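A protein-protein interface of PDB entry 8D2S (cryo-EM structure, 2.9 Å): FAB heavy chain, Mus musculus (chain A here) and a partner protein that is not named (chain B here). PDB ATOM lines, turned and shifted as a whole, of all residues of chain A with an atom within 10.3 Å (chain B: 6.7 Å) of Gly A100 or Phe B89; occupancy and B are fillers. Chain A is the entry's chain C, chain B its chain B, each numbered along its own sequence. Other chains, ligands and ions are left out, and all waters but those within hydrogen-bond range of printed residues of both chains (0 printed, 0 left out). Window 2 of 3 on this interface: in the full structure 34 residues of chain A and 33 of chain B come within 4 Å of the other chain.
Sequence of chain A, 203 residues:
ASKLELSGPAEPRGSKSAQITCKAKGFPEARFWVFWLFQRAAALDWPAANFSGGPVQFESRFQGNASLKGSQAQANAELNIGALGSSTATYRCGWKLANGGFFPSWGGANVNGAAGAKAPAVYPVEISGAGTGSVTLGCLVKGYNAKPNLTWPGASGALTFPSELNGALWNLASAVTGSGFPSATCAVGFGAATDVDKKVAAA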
ATOM      1  N   PHE A  32      -5.584 -16.624   4.275  1.00  0.00           N
ATOM      2  CA  PHE A  32      -5.308 -16.242   2.899  1.00  0.00           C
ATOM      3  C   PHE A  32      -5.982 -14.916   2.581  1.00  0.00           C
ATOM      4  O   PHE A  32      -6.967 -14.525   3.210  1.00  0.00           O
ATOM      5  CB  PHE A  32      -5.777 -17.319   1.911  1.00  0.00           C
ATOM      6  CG  PHE A  32      -5.034 -18.620   2.031  1.00  0.00           C
ATOM      7  CD1 PHE A  32      -3.882 -18.847   1.296  1.00  0.00           C
ATOM      8  CD2 PHE A  32      -5.488 -19.618   2.877  1.00  0.00           C
ATOM      9  CE1 PHE A  32      -3.199 -20.041   1.401  1.00  0.00           C
ATOM     10  CE2 PHE A  32      -4.808 -20.815   2.987  1.00  0.00           C
ATOM     11  CZ  PHE A  32      -3.663 -21.027   2.248  1.00  0.00           C
ATOM     12  N   TRP A  33      -5.425 -14.226   1.589  1.00  0.00           N
ATOM     13  CA  TRP A  33      -6.001 -12.996   1.064  1.00  0.00           C
ATOM     14  C   TRP A  33      -7.033 -13.348   0.001  1.00  0.00           C
ATOM     15  O   TRP A  33      -6.711 -14.021  -0.982  1.00  0.00           O
ATOM     16  CB  TRP A  33      -4.915 -12.102   0.464  1.00  0.00           C
ATOM     17  CG  TRP A  33      -4.020 -11.421   1.447  1.00  0.00           C
ATOM     18  CD1 TRP A  33      -2.933 -11.953   2.072  1.00  0.00           C
ATOM     19  CD2 TRP A  33      -4.116 -10.064   1.893  1.00  0.00           C
ATOM     20  NE1 TRP A  33      -2.354 -11.017   2.893  1.00  0.00           N
ATOM     21  CE2 TRP A  33      -3.062  -9.848   2.800  1.00  0.00           C
ATOM     22  CE3 TRP A  33      -4.996  -9.013   1.619  1.00  0.00           C
ATOM     23  CZ2 TRP A  33      -2.865  -8.625   3.435  1.00  0.00           C
ATOM     24  CZ3 TRP A  33      -4.799  -7.801   2.249  1.00  0.00           C
ATOM     25  CH2 TRP A  33      -3.742  -7.616   3.147  1.00  0.00           C
ATOM     26  N   PHE A  35      -9.458 -12.058  -2.956  1.00  0.00           N
ATOM     27  CA  PHE A  35      -9.341 -10.998  -3.939  1.00  0.00           C
ATOM     28  C   PHE A  35     -10.645 -10.838  -4.697  1.00  0.00           C
ATOM     29  O   PHE A  35     -11.358 -11.813  -4.944  1.00  0.00           O
ATOM     30  CB  PHE A  35      -8.227 -11.316  -4.933  1.00  0.00           C
ATOM     31  CG  PHE A  35      -6.864 -11.009  -4.423  1.00  0.00           C
ATOM     32  CD1 PHE A  35      -6.319 -11.715  -3.373  1.00  0.00           C
ATOM     33  CD2 PHE A  35      -6.125 -10.011  -5.001  1.00  0.00           C
ATOM     34  CE1 PHE A  35      -5.064 -11.410  -2.914  1.00  0.00           C
ATOM     35  CE2 PHE A  35      -4.874  -9.710  -4.550  1.00  0.00           C
ATOM     36  CZ  PHE A  35      -4.339 -10.414  -3.509  1.00  0.00           C
ATOM     37  N   TRP A  46      -8.766  -5.118 -11.181  1.00  0.00           N
ATOM     38  CA  TRP A  46      -8.426  -5.512  -9.816  1.00  0.00           C
ATOM     39  C   TRP A  46      -8.963  -4.487  -8.826  1.00  0.00           C
ATOM     40  O   TRP A  46      -8.295  -3.486  -8.534  1.00  0.00           O
ATOM     41  CB  TRP A  46      -6.915  -5.675  -9.664  1.00  0.00           C
ATOM     42  CG  TRP A  46      -6.506  -6.104  -8.303  1.00  0.00           C
ATOM     43  CD1 TRP A  46      -6.647  -7.343  -7.769  1.00  0.00           C
ATOM     44  CD2 TRP A  46      -5.885  -5.298  -7.293  1.00  0.00           C
ATOM     45  NE1 TRP A  46      -6.159  -7.362  -6.491  1.00  0.00           N
ATOM     46  CE2 TRP A  46      -5.683  -6.120  -6.172  1.00  0.00           C
ATOM     47  CE3 TRP A  46      -5.480  -3.962  -7.228  1.00  0.00           C
ATOM     48  CZ2 TRP A  46      -5.096  -5.657  -4.999  1.00  0.00           C
ATOM     49  CZ3 TRP A  46      -4.898  -3.502  -6.061  1.00  0.00           C
ATOM     50  CH2 TRP A  46      -4.711  -4.347  -4.963  1.00  0.00           C
ATOM     51  N   TRP A  95      -9.071 -16.609  -3.708  1.00  0.00           N
ATOM     52  CA  TRP A  95      -8.073 -16.511  -2.657  1.00  0.00           C
ATOM     53  C   TRP A  95      -6.680 -16.700  -3.241  1.00  0.00           C
ATOM     54  O   TRP A  95      -6.460 -17.549  -4.106  1.00  0.00           O
ATOM     55  CB  TRP A  95      -8.340 -17.525  -1.543  1.00  0.00           C
ATOM     56  CG  TRP A  95      -8.385 -18.952  -1.972  1.00  0.00           C
ATOM     57  CD1 TRP A  95      -9.416 -19.586  -2.601  1.00  0.00           C
ATOM     58  CD2 TRP A  95      -7.369 -19.939  -1.770  1.00  0.00           C
ATOM     59  NE1 TRP A  95      -9.097 -20.905  -2.818  1.00  0.00           N
ATOM     60  CE2 TRP A  95      -7.845 -21.146  -2.317  1.00  0.00           C
ATOM     61  CE3 TRP A  95      -6.100 -19.918  -1.188  1.00  0.00           C
ATOM     62  CZ2 TRP A  95      -7.096 -22.319  -2.298  1.00  0.00           C
ATOM     63  CZ3 TRP A  95      -5.359 -21.084  -1.170  1.00  0.00           C
ATOM     64  CH2 TRP A  95      -5.858 -22.267  -1.721  1.00  0.00           C
ATOM     65  N   LYS A  96      -5.746 -15.884  -2.767  1.00  0.00           N
ATOM     66  CA  LYS A  96      -4.381 -15.877  -3.265  1.00  0.00           C
ATOM     67  C   LYS A  96      -3.583 -17.024  -2.660  1.00  0.00           C
ATOM     68  O   LYS A  96      -3.891 -17.513  -1.570  1.00  0.00           O
ATOM     69  CB  LYS A  96      -3.713 -14.547  -2.915  1.00  0.00           C
ATOM     70  CG  LYS A  96      -2.464 -14.195  -3.696  1.00  0.00           C
ATOM     71  CD  LYS A  96      -1.781 -12.977  -3.091  1.00  0.00           C
ATOM     72  CE  LYS A  96      -1.315 -13.250  -1.669  1.00  0.00           C
ATOM     73  NZ  LYS A  96      -0.472 -12.156  -1.118  1.00  0.00           N
ATOM     74  N   LEU A  97      -2.556 -17.462  -3.384  1.00  0.00           N
ATOM     75  CA  LEU A  97      -1.554 -18.320  -2.769  1.00  0.00           C
ATOM     76  C   LEU A  97      -0.827 -17.539  -1.683  1.00  0.00           C
ATOM     77  O   LEU A  97      -0.522 -16.356  -1.849  1.00  0.00           O
ATOM     78  CB  LEU A  97      -0.555 -18.828  -3.810  1.00  0.00           C
ATOM     79  CG  LEU A  97       0.464 -19.820  -3.238  1.00  0.00           C
ATOM     80  CD1 LEU A  97      -0.156 -21.200  -3.070  1.00  0.00           C
ATOM     81  CD2 LEU A  97       1.740 -19.885  -4.056  1.00  0.00           C
ATOM     82  N   ALA A  98      -0.548 -18.208  -0.561  1.00  0.00           N
ATOM     83  CA  ALA A  98       0.076 -17.535   0.573  1.00  0.00           C
ATOM     84  C   ALA A  98       1.497 -17.071   0.279  1.00  0.00           C
ATOM     85  O   ALA A  98       2.034 -16.258   1.038  1.00  0.00           O
ATOM     86  CB  ALA A  98       0.077 -18.456   1.793  1.00  0.00           C
ATOM     87  N   ASN A  99       2.113 -17.555  -0.796  1.00  0.00           N
ATOM     88  CA  ASN A  99       3.505 -17.250  -1.099  1.00  0.00           C
ATOM     89  C   ASN A  99       3.705 -16.468  -2.387  1.00  0.00           C
ATOM     90  O   ASN A  99       4.498 -15.525  -2.409  1.00  0.00           O
ATOM     91  CB  ASN A  99       4.313 -18.550  -1.175  1.00  0.00           C
ATOM     92  CG  ASN A  99       4.036 -19.476  -0.008  1.00  0.00           C
ATOM     93  OD1 ASN A  99       3.580 -20.602  -0.190  1.00  0.00           O
ATOM     94  ND2 ASN A  99       4.307 -19.004   1.203  1.00  0.00           N
ATOM     95  N   GLY A 100       3.004 -16.822  -3.461  1.00  0.00           N
ATOM     96  CA  GLY A 100       3.336 -16.315  -4.778  1.00  0.00           C
ATOM     97  C   GLY A 100       2.771 -14.957  -5.140  1.00  0.00           C
ATOM     98  O   GLY A 100       3.523 -14.042  -5.489  1.00  0.00           O
ATOM     99  N   GLY A 101       1.452 -14.808  -5.062  1.00  0.00           N
ATOM    100  CA  GLY A 101       0.781 -13.612  -5.544  1.00  0.00           C
ATOM    101  C   GLY A 101      -0.195 -13.849  -6.678  1.00  0.00           C
ATOM    102  O   GLY A 101      -0.778 -12.879  -7.182  1.00  0.00           O
ATOM    103  N   PHE A 102      -0.398 -15.089  -7.109  1.00  0.00           N
ATOM    104  CA  PHE A 102      -1.371 -15.437  -8.132  1.00  0.00           C
ATOM    105  C   PHE A 102      -2.608 -16.057  -7.487  1.00  0.00           C
ATOM    106  O   PHE A 102      -2.632 -16.355  -6.291  1.00  0.00           O
ATOM    107  CB  PHE A 102      -0.753 -16.388  -9.163  1.00  0.00           C
ATOM    108  CG  PHE A 102      -0.123 -17.618  -8.563  1.00  0.00           C
ATOM    109  CD1 PHE A 102       1.201 -17.609  -8.157  1.00  0.00           C
ATOM    110  CD2 PHE A 102      -0.854 -18.784  -8.419  1.00  0.00           C
ATOM    111  CE1 PHE A 102       1.777 -18.735  -7.606  1.00  0.00           C
ATOM    112  CE2 PHE A 102      -0.283 -19.913  -7.871  1.00  0.00           C
ATOM    113  CZ  PHE A 102       1.034 -19.890  -7.471  1.00  0.00           C
ATOM    114  N   PHE A 103      -3.647 -16.247  -8.297  1.00  0.00           N
ATOM    115  CA  PHE A 103      -4.947 -16.669  -7.783  1.00  0.00           C
ATOM    116  C   PHE A 103      -5.266 -18.082  -8.256  1.00  0.00           C
ATOM    117  O   PHE A 103      -5.618 -18.268  -9.430  1.00  0.00           O
ATOM    118  CB  PHE A 103      -6.045 -15.701  -8.233  1.00  0.00           C
ATOM    119  CG  PHE A 103      -5.667 -14.246  -8.123  1.00  0.00           C
ATOM    120  CD1 PHE A 103      -5.017 -13.757  -7.001  1.00  0.00           C
ATOM    121  CD2 PHE A 103      -5.967 -13.365  -9.149  1.00  0.00           C
ATOM    122  CE1 PHE A 103      -4.665 -12.428  -6.911  1.00  0.00           C
ATOM    123  CE2 PHE A 103      -5.623 -12.030  -9.060  1.00  0.00           C
ATOM    124  CZ  PHE A 103      -4.973 -11.561  -7.941  1.00  0.00           C
ATOM    125  N   PRO A 104      -5.158 -19.103  -7.395  1.00  0.00           N
ATOM    126  CA  PRO A 104      -5.494 -20.471  -7.818  1.00  0.00           C
ATOM    127  C   PRO A 104      -6.971 -20.680  -8.119  1.00  0.00           C
ATOM    128  O   PRO A 104      -7.321 -21.192  -9.186  1.00  0.00           O
ATOM    129  CB  PRO A 104      -5.052 -21.322  -6.621  1.00  0.00           C
ATOM    130  CG  PRO A 104      -4.041 -20.494  -5.911  1.00  0.00           C
ATOM    131  CD  PRO A 104      -4.491 -19.080  -6.085  1.00  0.00           C
ATOM    132  N   VAL B  28       9.789  -7.621 -14.035  1.00  0.00           N
ATOM    133  CA  VAL B  28       9.018  -8.244 -12.963  1.00  0.00           C
ATOM    134  C   VAL B  28       9.687  -9.483 -12.385  1.00  0.00           C
ATOM    135  O   VAL B  28       9.115 -10.119 -11.489  1.00  0.00           O
ATOM    136  CB  VAL B  28       7.596  -8.604 -13.442  1.00  0.00           C
ATOM    137  CG1 VAL B  28       6.817  -7.345 -13.782  1.00  0.00           C
ATOM    138  CG2 VAL B  28       7.658  -9.534 -14.634  1.00  0.00           C
ATOM    139  N   SER B  30      10.374 -12.598 -13.607  1.00  0.00           N
ATOM    140  CA  SER B  30       9.707 -13.868 -13.920  1.00  0.00           C
ATOM    141  C   SER B  30       8.521 -14.144 -13.000  1.00  0.00           C
ATOM    142  O   SER B  30       8.157 -15.298 -12.769  1.00  0.00           O
ATOM    143  CB  SER B  30      10.687 -15.048 -13.895  1.00  0.00           C
ATOM    144  OG  SER B  30      11.055 -15.385 -12.570  1.00  0.00           O
ATOM    145  N   ALA B  31       7.905 -13.092 -12.469  1.00  0.00           N
ATOM    146  CA  ALA B  31       6.723 -13.231 -11.623  1.00  0.00           C
ATOM    147  C   ALA B  31       5.465 -12.988 -12.456  1.00  0.00           C
ATOM    148  O   ALA B  31       4.744 -12.004 -12.292  1.00  0.00           O
ATOM    149  CB  ALA B  31       6.807 -12.279 -10.435  1.00  0.00           C
ATOM    150  N   VAL B  32       5.213 -13.921 -13.374  1.00  0.00           N
ATOM    151  CA  VAL B  32       4.107 -13.823 -14.318  1.00  0.00           C
ATOM    152  C   VAL B  32       3.300 -15.113 -14.276  1.00  0.00           C
ATOM    153  O   VAL B  32       3.857 -16.205 -14.434  1.00  0.00           O
ATOM    154  CB  VAL B  32       4.603 -13.539 -15.749  1.00  0.00           C
ATOM    155  CG1 VAL B  32       3.477 -13.712 -16.753  1.00  0.00           C
ATOM    156  CG2 VAL B  32       5.164 -12.137 -15.835  1.00  0.00           C
ATOM    157  N   ALA B  33       1.997 -14.982 -14.059  1.00  0.00           N
ATOM    158  CA  ALA B  33       1.055 -16.088 -14.121  1.00  0.00           C
ATOM    159  C   ALA B  33       0.244 -16.015 -15.409  1.00  0.00           C
ATOM    160  O   ALA B  33       0.052 -14.943 -15.985  1.00  0.00           O
ATOM    161  CB  ALA B  33       0.116 -16.077 -12.913  1.00  0.00           C
ATOM    162  N   TRP B  34      -0.225 -17.173 -15.855  1.00  0.00           N
ATOM    163  CA  TRP B  34      -1.059 -17.302 -17.041  1.00  0.00           C
ATOM    164  C   TRP B  34      -2.345 -18.013 -16.660  1.00  0.00           C
ATOM    165  O   TRP B  34      -2.301 -19.105 -16.082  1.00  0.00           O
ATOM    166  CB  TRP B  34      -0.342 -18.077 -18.151  1.00  0.00           C
ATOM    167  CG  TRP B  34       0.700 -17.284 -18.867  1.00  0.00           C
ATOM    168  CD1 TRP B  34       2.036 -17.259 -18.603  1.00  0.00           C
ATOM    169  CD2 TRP B  34       0.491 -16.399 -19.972  1.00  0.00           C
ATOM    170  NE1 TRP B  34       2.674 -16.411 -19.474  1.00  0.00           N
ATOM    171  CE2 TRP B  34       1.746 -15.870 -20.326  1.00  0.00           C
ATOM    172  CE3 TRP B  34      -0.637 -16.002 -20.698  1.00  0.00           C
ATOM    173  CZ2 TRP B  34       1.908 -14.967 -21.372  1.00  0.00           C
ATOM    174  CZ3 TRP B  34      -0.475 -15.105 -21.736  1.00  0.00           C
ATOM    175  CH2 TRP B  34       0.787 -14.597 -22.063  1.00  0.00           C
ATOM    176  N   THR B  47      -0.364 -21.301 -15.480  1.00  0.00           N
ATOM    177  CA  THR B  47       1.062 -21.227 -15.205  1.00  0.00           C
ATOM    178  C   THR B  47       1.316 -20.174 -14.138  1.00  0.00           C
ATOM    179  O   THR B  47       0.593 -19.183 -14.046  1.00  0.00           O
ATOM    180  CB  THR B  47       1.862 -20.901 -16.484  1.00  0.00           C
ATOM    181  OG1 THR B  47       1.373 -21.700 -17.567  1.00  0.00           O
ATOM    182  CG2 THR B  47       3.340 -21.201 -16.297  1.00  0.00           C
ATOM    183  N   TYR B  48       2.333 -20.406 -13.314  1.00  0.00           N
ATOM    184  CA  TYR B  48       2.775 -19.407 -12.357  1.00  0.00           C
ATOM    185  C   TYR B  48       4.295 -19.390 -12.325  1.00  0.00           C
ATOM    186  O   TYR B  48       4.954 -20.382 -12.643  1.00  0.00           O
ATOM    187  CB  TYR B  48       2.196 -19.657 -10.961  1.00  0.00           C
ATOM    188  CG  TYR B  48       2.390 -21.056 -10.420  1.00  0.00           C
ATOM    189  CD1 TYR B  48       1.461 -22.054 -10.677  1.00  0.00           C
ATOM    190  CD2 TYR B  48       3.487 -21.368  -9.629  1.00  0.00           C
ATOM    191  CE1 TYR B  48       1.630 -23.328 -10.177  1.00  0.00           C
ATOM    192  CE2 TYR B  48       3.661 -22.638  -9.123  1.00  0.00           C
ATOM    193  CZ  TYR B  48       2.731 -23.615  -9.401  1.00  0.00           C
ATOM    194  OH  TYR B  48       2.901 -24.884  -8.900  1.00  0.00           O
ATOM    195  N   TRP B  49       4.838 -18.228 -11.948  1.00  0.00           N
ATOM    196  CA  TRP B  49       6.275 -17.939 -11.991  1.00  0.00           C
ATOM    197  C   TRP B  49       6.857 -18.156 -13.386  1.00  0.00           C
ATOM    198  O   TRP B  49       8.016 -18.554 -13.529  1.00  0.00           O
ATOM    199  CB  TRP B  49       7.050 -18.754 -10.949  1.00  0.00           C
ATOM    200  CG  TRP B  49       6.896 -18.232  -9.555  1.00  0.00           C
ATOM    201  CD1 TRP B  49       6.153 -18.780  -8.552  1.00  0.00           C
ATOM    202  CD2 TRP B  49       7.496 -17.051  -9.012  1.00  0.00           C
ATOM    203  NE1 TRP B  49       6.256 -18.016  -7.416  1.00  0.00           N
ATOM    204  CE2 TRP B  49       7.074 -16.948  -7.673  1.00  0.00           C
ATOM    205  CE3 TRP B  49       8.349 -16.072  -9.528  1.00  0.00           C
ATOM    206  CZ2 TRP B  49       7.477 -15.905  -6.843  1.00  0.00           C
ATOM    207  CZ3 TRP B  49       8.749 -15.039  -8.704  1.00  0.00           C
ATOM    208  CH2 TRP B  49       8.313 -14.964  -7.375  1.00  0.00           C
ATOM    209  N   ALA B  50       6.024 -17.942 -14.410  1.00  0.00           N
ATOM    210  CA  ALA B  50       6.386 -17.902 -15.826  1.00  0.00           C
ATOM    211  C   ALA B  50       6.837 -19.248 -16.385  1.00  0.00           C
ATOM    212  O   ALA B  50       7.122 -19.350 -17.582  1.00  0.00           O
ATOM    213  CB  ALA B  50       7.469 -16.847 -16.080  1.00  0.00           C
ATOM    214  N   LEU B  87      -1.021 -12.294 -15.784  1.00  0.00           N
ATOM    215  CA  LEU B  87      -1.019 -11.505 -14.563  1.00  0.00           C
ATOM    216  C   LEU B  87       0.411 -11.334 -14.066  1.00  0.00           C
ATOM    217  O   LEU B  87       1.245 -12.227 -14.218  1.00  0.00           O
ATOM    218  CB  LEU B  87      -1.873 -12.185 -13.483  1.00  0.00           C
ATOM    219  CG  LEU B  87      -1.832 -11.661 -12.046  1.00  0.00           C
ATOM    220  CD1 LEU B  87      -2.398 -10.271 -12.007  1.00  0.00           C
ATOM    221  CD2 LEU B  87      -2.567 -12.566 -11.070  1.00  0.00           C
ATOM    222  N   LEU B  88       0.695 -10.178 -13.481  1.00  0.00           N
ATOM    223  CA  LEU B  88       1.935  -9.979 -12.749  1.00  0.00           C
ATOM    224  C   LEU B  88       1.689 -10.214 -11.263  1.00  0.00           C
ATOM    225  O   LEU B  88       0.603  -9.944 -10.748  1.00  0.00           O
ATOM    226  CB  LEU B  88       2.492  -8.569 -12.972  1.00  0.00           C
ATOM    227  CG  LEU B  88       1.802  -7.389 -12.277  1.00  0.00           C
ATOM    228  CD1 LEU B  88       2.622  -6.887 -11.100  1.00  0.00           C
ATOM    229  CD2 LEU B  88       1.531  -6.264 -13.253  1.00  0.00           C
ATOM    230  N   PHE B  89       2.696 -10.745 -10.579  1.00  0.00           N
ATOM    231  CA  PHE B  89       2.697 -10.752  -9.121  1.00  0.00           C
ATOM    232  C   PHE B  89       4.066 -10.314  -8.615  1.00  0.00           C
ATOM    233  O   PHE B  89       4.658 -10.919  -7.721  1.00  0.00           O
ATOM    234  CB  PHE B  89       2.265 -12.102  -8.543  1.00  0.00           C
ATOM    235  CG  PHE B  89       2.911 -13.298  -9.181  1.00  0.00           C
ATOM    236  CD1 PHE B  89       2.339 -13.906 -10.284  1.00  0.00           C
ATOM    237  CD2 PHE B  89       4.061 -13.850  -8.643  1.00  0.00           C
ATOM    238  CE1 PHE B  89       2.922 -15.016 -10.857  1.00  0.00           C
ATOM    239  CE2 PHE B  89       4.644 -14.959  -9.213  1.00  0.00           C
ATOM    240  CZ  PHE B  89       4.074 -15.541 -10.319  1.00  0.00           C
ATOM    241  N   GLU B  90       4.579  -9.234  -9.203  1.00  0.00           N
ATOM    242  CA  GLU B  90       5.791  -8.572  -8.740  1.00  0.00           C
ATOM    243  C   GLU B  90       5.479  -7.478  -7.722  1.00  0.00           C
ATOM    244  O   GLU B  90       6.139  -7.386  -6.684  1.00  0.00           O
ATOM    245  CB  GLU B  90       6.554  -7.991  -9.938  1.00  0.00           C
ATOM    246  CG  GLU B  90       7.538  -6.873  -9.603  1.00  0.00           C
ATOM    247  CD  GLU B  90       8.894  -7.384  -9.155  1.00  0.00           C
ATOM    248  OE1 GLU B  90       9.064  -8.614  -9.032  1.00  0.00           O
ATOM    249  OE2 GLU B  90       9.797  -6.551  -8.929  1.00  0.00           O
ATOM    250  N   LYS B  91       4.470  -6.655  -8.000  1.00  0.00           N
ATOM    251  CA  LYS B  91       4.069  -5.576  -7.113  1.00  0.00           C
ATOM    252  C   LYS B  91       2.613  -5.754  -6.702  1.00  0.00           C
ATOM    253  O   LYS B  91       1.860  -6.513  -7.316  1.00  0.00           O
ATOM    254  CB  LYS B  91       4.275  -4.206  -7.768  1.00  0.00           C
ATOM    255  CG  LYS B  91       5.727  -3.909  -8.098  1.00  0.00           C
ATOM    256  CD  LYS B  91       6.078  -2.457  -7.831  1.00  0.00           C
ATOM    257  CE  LYS B  91       7.537  -2.180  -8.156  1.00  0.00           C
ATOM    258  NZ  LYS B  91       7.912  -0.766  -7.880  1.00  0.00           N
ATOM    259  N   GLY B  92       2.229  -5.031  -5.645  1.00  0.00           N
ATOM    260  CA  GLY B  92       0.956  -5.278  -4.988  1.00  0.00           C
ATOM    261  C   GLY B  92      -0.258  -5.003  -5.850  1.00  0.00           C
ATOM    262  O   GLY B  92      -1.270  -5.702  -5.737  1.00  0.00           O
ATOM    263  N   PHE B  94      -2.131  -5.555  -8.966  1.00  0.00           N
ATOM    264  CA  PHE B  94      -2.058  -6.635  -9.939  1.00  0.00           C
ATOM    265  C   PHE B  94      -2.803  -6.265 -11.220  1.00  0.00           C
ATOM    266  O   PHE B  94      -3.861  -5.633 -11.174  1.00  0.00           O
ATOM    267  CB  PHE B  94      -2.625  -7.917  -9.329  1.00  0.00           C
ATOM    268  CG  PHE B  94      -1.884  -8.382  -8.100  1.00  0.00           C
ATOM    269  CD1 PHE B  94      -0.540  -8.711  -8.170  1.00  0.00           C
ATOM    270  CD2 PHE B  94      -2.529  -8.493  -6.880  1.00  0.00           C
ATOM    271  CE1 PHE B  94       0.148  -9.139  -7.050  1.00  0.00           C
ATOM    272  CE2 PHE B  94      -1.841  -8.919  -5.756  1.00  0.00           C
ATOM    273  CZ  PHE B  94      -0.504  -9.243  -5.842  1.00  0.00           C
ATOM    274  N   SER B  95      -2.240  -6.663 -12.365  1.00  0.00           N
ATOM    275  CA  SER B  95      -2.728  -6.221 -13.664  1.00  0.00           C
ATOM    276  C   SER B  95      -2.743  -7.377 -14.658  1.00  0.00           C
ATOM    277  O   SER B  95      -1.953  -8.317 -14.550  1.00  0.00           O
ATOM    278  CB  SER B  95      -1.867  -5.077 -14.213  1.00  0.00           C
ATOM    279  OG  SER B  95      -1.684  -4.066 -13.237  1.00  0.00           O
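The backbone NH (N) of Phe B89 is in hydrogen-bond range of the backbone carbonyl oxygen (O) of Ala B31 (3.0 Å). The backbone NH (N) of Ala B33 is in hydrogen-bond range of the backbone carbonyl oxygen (O) of Leu B87, 2.9 Å away. N of Leu A97 lies within hydrogen-bond range of O of Phe A102.
Among the printed residues, merely in contact across the chains: Gly A100 with Phe B89, Phe A35 with Phe B94, Trp A46 with Phe B94, Gly A101 with Phe B89, Phe A102 with Tyr B48, Phe A103 with Leu B87, Trp A46 with Gly B92, Gly A101 with Phe B94 and Phe A102 with Ala B33.
Of the 14 printed residues of chain A, 6 touch a printed residue of chain B. Hydrophobic or aromatic side chains of chain A that line the printed part of chain B: Phe A35, Trp A46, Phe A102 and Phe A103. Among the printed residues, no Asp or Glu carboxylate lies within 4 Å of a Lys or Arg side-chain nitrogen of the other chain.
Gly A100 touches just one residue of chain B: Phe B89 (3.2 Å). Phe B89 touches just these residues of chain A: Gly A100 and Gly A101. No residue of chain A comes within 4 Å of Leu B88. Of the printed residues of chain A, Phe B94 touches Phe A35, Trp A46 and Gly A101. Of the printed residues of chain B, Gly A101 touches Phe B89 and Phe B94. Printed residues of chain B within 4 Å of Trp A46: Gly B92 (3.8 Å) and Phe B94 (3.4 Å). Of the printed residues of chain B, Phe A103 touches Leu B87 (3.7 Å). Ala B50 touches none of the printed residues of chain A. Lys B91 touches none of the printed residues of chain A. The nearest residue of chain A that does not touch Phe B89 is Phe A102 (4.1 Å). The nearest printed residue of chain A that does not touch Phe B94 is Phe A103 (4.1 Å).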
